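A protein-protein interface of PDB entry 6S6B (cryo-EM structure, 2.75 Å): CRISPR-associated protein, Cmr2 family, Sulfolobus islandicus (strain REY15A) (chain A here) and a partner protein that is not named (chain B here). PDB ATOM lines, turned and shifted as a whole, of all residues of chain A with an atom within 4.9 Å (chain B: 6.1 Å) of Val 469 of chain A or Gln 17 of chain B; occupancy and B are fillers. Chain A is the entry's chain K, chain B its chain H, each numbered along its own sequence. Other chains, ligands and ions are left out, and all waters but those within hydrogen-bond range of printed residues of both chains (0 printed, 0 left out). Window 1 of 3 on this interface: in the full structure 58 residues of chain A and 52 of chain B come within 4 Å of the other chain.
Val 469 of chain A touches two residues of chain B.
Of chain A, only Cys 467, Gly 468, Val 469 and Phe 871 come within 4 Å of Gln 17 of chain B.
Printed residues of chain A within 4 Å of Glu 19 of chain B: Phe 463 (3.2 Å).
Printed residues of chain B within 4 Å of Pro 471 of chain A: Met 259 (3.6 Å).
Of the printed residues of chain B, Phe 463 of chain A touches Gly 18 (3.4 Å), Glu 19 (3.2 Å) and Met 259 (3.4 Å).
The nearest residue of chain B that does not touch Val 469 of chain A is Lys 244 of chain B (5.0 Å).
Among the printed residues, pairs that only touch across the chains: Glu 436 of chain A with Lys 244 of chain B (3.3 Å), Phe 463 of chain A with Gly 18 of chain B (3.4 Å), Phe 463 of chain A with Met 259 of chain B (3.4 Å), Cys 467 of chain A with Gln 17 of chain B (3.6 Å), Val 469 of chain A with Gln 17 of chain B (3.4 Å), Pro 471 of chain A with Met 259 of chain B (3.6 Å) and Phe 871 of chain A with Gln 17 of chain B (3.8 Å).
Hydrophobic or aromatic side chains of chain B that line the printed part of chain A: Met 259.
Of the 8 printed residues of chain A, 7 touch a printed residue of chain B.
Hydrophobic or aromatic side chains of chain A that line the printed part of chain B: Phe 463, Val 469, Pro 471 and Phe 871.
Among the printed residues, no Asp or Glu carboxylate lies within 4 Å of a Lys or Arg side-chain nitrogen of the other chain.
O of Gly 468 of chain A lies close to O of Gln 17 of chain B, at 2.6 Å.
OE2 of Glu 19 of chain B lies within hydrogen-bond range of N of Phe 463 of chain A (3.3 Å).
O of Val 469 of chain A sits close to SD of Met 259 of chain B.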
ATOM      1  N   GLU A 436     -19.225 -27.696   7.861  1.00  0.00           N
ATOM      2  CA  GLU A 436     -20.480 -27.166   7.346  1.00  0.00           C
ATOM      3  C   GLU A 436     -20.265 -26.219   6.181  1.00  0.00           C
ATOM      4  O   GLU A 436     -21.198 -25.985   5.408  1.00  0.00           O
ATOM      5  CB  GLU A 436     -21.242 -26.442   8.452  1.00  0.00           C
ATOM      6  CG  GLU A 436     -21.846 -27.360   9.484  1.00  0.00           C
ATOM      7  CD  GLU A 436     -20.823 -27.907  10.452  1.00  0.00           C
ATOM      8  OE1 GLU A 436     -19.691 -27.387  10.476  1.00  0.00           O
ATOM      9  OE2 GLU A 436     -21.150 -28.859  11.190  1.00  0.00           O
ATOM     10  N   PHE A 463     -33.267 -23.787  12.323  1.00  0.00           N
ATOM     11  CA  PHE A 463     -32.001 -24.470  12.594  1.00  0.00           C
ATOM     12  C   PHE A 463     -32.140 -25.765  13.388  1.00  0.00           C
ATOM     13  O   PHE A 463     -33.060 -25.917  14.193  1.00  0.00           O
ATOM     14  CB  PHE A 463     -31.053 -23.574  13.392  1.00  0.00           C
ATOM     15  CG  PHE A 463     -30.698 -22.298  12.719  1.00  0.00           C
ATOM     16  CD1 PHE A 463     -29.923 -22.294  11.584  1.00  0.00           C
ATOM     17  CD2 PHE A 463     -31.110 -21.096  13.244  1.00  0.00           C
ATOM     18  CE1 PHE A 463     -29.585 -21.114  10.978  1.00  0.00           C
ATOM     19  CE2 PHE A 463     -30.770 -19.917  12.644  1.00  0.00           C
ATOM     20  CZ  PHE A 463     -30.011 -19.926  11.507  1.00  0.00           C
ATOM     21  N   CYS A 467     -26.954 -29.571  16.016  1.00  0.00           N
ATOM     22  CA  CYS A 467     -25.915 -28.690  15.497  1.00  0.00           C
ATOM     23  C   CYS A 467     -26.127 -27.256  15.955  1.00  0.00           C
ATOM     24  O   CYS A 467     -25.310 -26.692  16.691  1.00  0.00           O
ATOM     25  CB  CYS A 467     -25.879 -28.749  13.969  1.00  0.00           C
ATOM     26  SG  CYS A 467     -25.185 -30.242  13.261  1.00  0.00           S
ATOM     27  N   GLY A 468     -27.229 -26.651  15.531  1.00  0.00           N
ATOM     28  CA  GLY A 468     -27.401 -25.226  15.610  1.00  0.00           C
ATOM     29  C   GLY A 468     -27.000 -24.481  14.356  1.00  0.00           C
ATOM     30  O   GLY A 468     -27.463 -23.361  14.141  1.00  0.00           O
ATOM     31  N   VAL A 469     -26.164 -25.071  13.513  1.00  0.00           N
ATOM     32  CA  VAL A 469     -25.694 -24.379  12.321  1.00  0.00           C
ATOM     33  C   VAL A 469     -26.562 -24.693  11.109  1.00  0.00           C
ATOM     34  O   VAL A 469     -26.999 -23.787  10.397  1.00  0.00           O
ATOM     35  CB  VAL A 469     -24.206 -24.709  12.074  1.00  0.00           C
ATOM     36  CG1 VAL A 469     -23.356 -24.084  13.156  1.00  0.00           C
ATOM     37  CG2 VAL A 469     -23.981 -26.202  12.079  1.00  0.00           C
ATOM     38  N   LEU A 470     -26.844 -25.959  10.854  1.00  0.00           N
ATOM     39  CA  LEU A 470     -27.571 -26.304   9.646  1.00  0.00           C
ATOM     40  C   LEU A 470     -29.075 -26.168   9.854  1.00  0.00           C
ATOM     41  O   LEU A 470     -29.571 -26.328  10.971  1.00  0.00           O
ATOM     42  CB  LEU A 470     -27.249 -27.727   9.224  1.00  0.00           C
ATOM     43  CG  LEU A 470     -25.776 -28.009   8.968  1.00  0.00           C
ATOM     44  CD1 LEU A 470     -25.615 -29.387   8.381  1.00  0.00           C
ATOM     45  CD2 LEU A 470     -25.211 -26.961   8.041  1.00  0.00           C
ATOM     46  N   PRO A 471     -29.822 -25.869   8.796  1.00  0.00           N
ATOM     47  CA  PRO A 471     -31.280 -25.888   8.899  1.00  0.00           C
ATOM     48  C   PRO A 471     -31.777 -27.303   9.129  1.00  0.00           C
ATOM     49  O   PRO A 471     -31.094 -28.286   8.844  1.00  0.00           O
ATOM     50  CB  PRO A 471     -31.748 -25.350   7.544  1.00  0.00           C
ATOM     51  CG  PRO A 471     -30.542 -24.760   6.908  1.00  0.00           C
ATOM     52  CD  PRO A 471     -29.376 -25.511   7.442  1.00  0.00           C
ATOM     53  N   PHE A 871     -24.340 -29.376  23.943  1.00  0.00           N
ATOM     54  CA  PHE A 871     -23.437 -28.646  23.065  1.00  0.00           C
ATOM     55  C   PHE A 871     -22.550 -27.703  23.859  1.00  0.00           C
ATOM     56  O   PHE A 871     -21.342 -27.625  23.615  1.00  0.00           O
ATOM     57  CB  PHE A 871     -24.232 -27.873  22.016  1.00  0.00           C
ATOM     58  CG  PHE A 871     -23.398 -26.946  21.182  1.00  0.00           C
ATOM     59  CD1 PHE A 871     -22.755 -27.405  20.051  1.00  0.00           C
ATOM     60  CD2 PHE A 871     -23.271 -25.615  21.522  1.00  0.00           C
ATOM     61  CE1 PHE A 871     -21.993 -26.556  19.284  1.00  0.00           C
ATOM     62  CE2 PHE A 871     -22.511 -24.765  20.757  1.00  0.00           C
ATOM     63  CZ  PHE A 871     -21.873 -25.235  19.637  1.00  0.00           C
ATOM     64  N   ARG B  15     -26.147 -13.415  19.247  1.00  0.00           N
ATOM     65  CA  ARG B  15     -25.993 -14.858  19.243  1.00  0.00           C
ATOM     66  C   ARG B  15     -25.951 -15.386  17.821  1.00  0.00           C
ATOM     67  O   ARG B  15     -26.595 -14.845  16.920  1.00  0.00           O
ATOM     68  CB  ARG B  15     -27.125 -15.536  20.008  1.00  0.00           C
ATOM     69  CG  ARG B  15     -28.461 -15.445  19.342  1.00  0.00           C
ATOM     70  CD  ARG B  15     -29.528 -16.124  20.171  1.00  0.00           C
ATOM     71  NE  ARG B  15     -30.846 -15.954  19.578  1.00  0.00           N
ATOM     72  CZ  ARG B  15     -31.367 -16.794  18.696  1.00  0.00           C
ATOM     73  NH1 ARG B  15     -32.573 -16.576  18.195  1.00  0.00           N
ATOM     74  NH2 ARG B  15     -30.680 -17.860  18.326  1.00  0.00           N
ATOM     75  N   SER B  16     -25.177 -16.433  17.631  1.00  0.00           N
ATOM     76  CA  SER B  16     -25.203 -17.231  16.425  1.00  0.00           C
ATOM     77  C   SER B  16     -25.876 -18.562  16.745  1.00  0.00           C
ATOM     78  O   SER B  16     -26.451 -18.745  17.823  1.00  0.00           O
ATOM     79  CB  SER B  16     -23.785 -17.404  15.894  1.00  0.00           C
ATOM     80  OG  SER B  16     -22.993 -18.112  16.828  1.00  0.00           O
ATOM     81  N   GLN B  17     -25.855 -19.484  15.787  1.00  0.00           N
ATOM     82  CA  GLN B  17     -26.220 -20.879  16.017  1.00  0.00           C
ATOM     83  C   GLN B  17     -27.717 -21.084  16.216  1.00  0.00           C
ATOM     84  O   GLN B  17     -28.175 -22.225  16.316  1.00  0.00           O
ATOM     85  CB  GLN B  17     -25.472 -21.449  17.229  1.00  0.00           C
ATOM     86  CG  GLN B  17     -23.983 -21.212  17.222  1.00  0.00           C
ATOM     87  CD  GLN B  17     -23.246 -22.278  16.462  1.00  0.00           C
ATOM     88  OE1 GLN B  17     -22.374 -21.984  15.646  1.00  0.00           O
ATOM     89  NE2 GLN B  17     -23.596 -23.533  16.716  1.00  0.00           N
ATOM     90  N   GLY B  18     -28.486 -20.006  16.299  1.00  0.00           N
ATOM     91  CA  GLY B  18     -29.932 -20.119  16.266  1.00  0.00           C
ATOM     92  C   GLY B  18     -30.573 -20.972  17.343  1.00  0.00           C
ATOM     93  O   GLY B  18     -29.885 -21.584  18.161  1.00  0.00           O
ATOM     94  N   GLU B  19     -31.905 -21.023  17.341  1.00  0.00           N
ATOM     95  CA  GLU B  19     -32.679 -21.915  18.201  1.00  0.00           C
ATOM     96  C   GLU B  19     -32.371 -21.666  19.679  1.00  0.00           C
ATOM     97  O   GLU B  19     -31.806 -22.497  20.389  1.00  0.00           O
ATOM     98  CB  GLU B  19     -32.443 -23.379  17.824  1.00  0.00           C
ATOM     99  CG  GLU B  19     -32.933 -23.702  16.437  1.00  0.00           C
ATOM    100  CD  GLU B  19     -34.298 -23.117  16.160  1.00  0.00           C
ATOM    101  OE1 GLU B  19     -35.209 -23.307  16.990  1.00  0.00           O
ATOM    102  OE2 GLU B  19     -34.458 -22.450  15.118  1.00  0.00           O
ATOM    103  N   LYS B 244     -19.784 -21.856   7.721  1.00  0.00           N
ATOM    104  CA  LYS B 244     -21.059 -21.484   7.135  1.00  0.00           C
ATOM    105  C   LYS B 244     -21.869 -20.686   8.143  1.00  0.00           C
ATOM    106  O   LYS B 244     -22.090 -21.141   9.268  1.00  0.00           O
ATOM    107  CB  LYS B 244     -21.835 -22.719   6.693  1.00  0.00           C
ATOM    108  CG  LYS B 244     -23.078 -22.390   5.914  1.00  0.00           C
ATOM    109  CD  LYS B 244     -23.447 -23.514   4.981  1.00  0.00           C
ATOM    110  CE  LYS B 244     -22.580 -23.502   3.743  1.00  0.00           C
ATOM    111  NZ  LYS B 244     -22.913 -22.364   2.852  1.00  0.00           N
ATOM    112  N   MET B 259     -28.042 -18.660   4.153  1.00  0.00           N
ATOM    113  CA  MET B 259     -26.921 -19.290   4.832  1.00  0.00           C
ATOM    114  C   MET B 259     -25.861 -19.618   3.797  1.00  0.00           C
ATOM    115  O   MET B 259     -26.071 -20.492   2.952  1.00  0.00           O
ATOM    116  CB  MET B 259     -27.363 -20.553   5.566  1.00  0.00           C
ATOM    117  CG  MET B 259     -26.305 -21.146   6.456  1.00  0.00           C
ATOM    118  SD  MET B 259     -26.894 -22.628   7.270  1.00  0.00           S
ATOM    119  CE  MET B 259     -28.451 -22.022   7.877  1.00  0.00           C
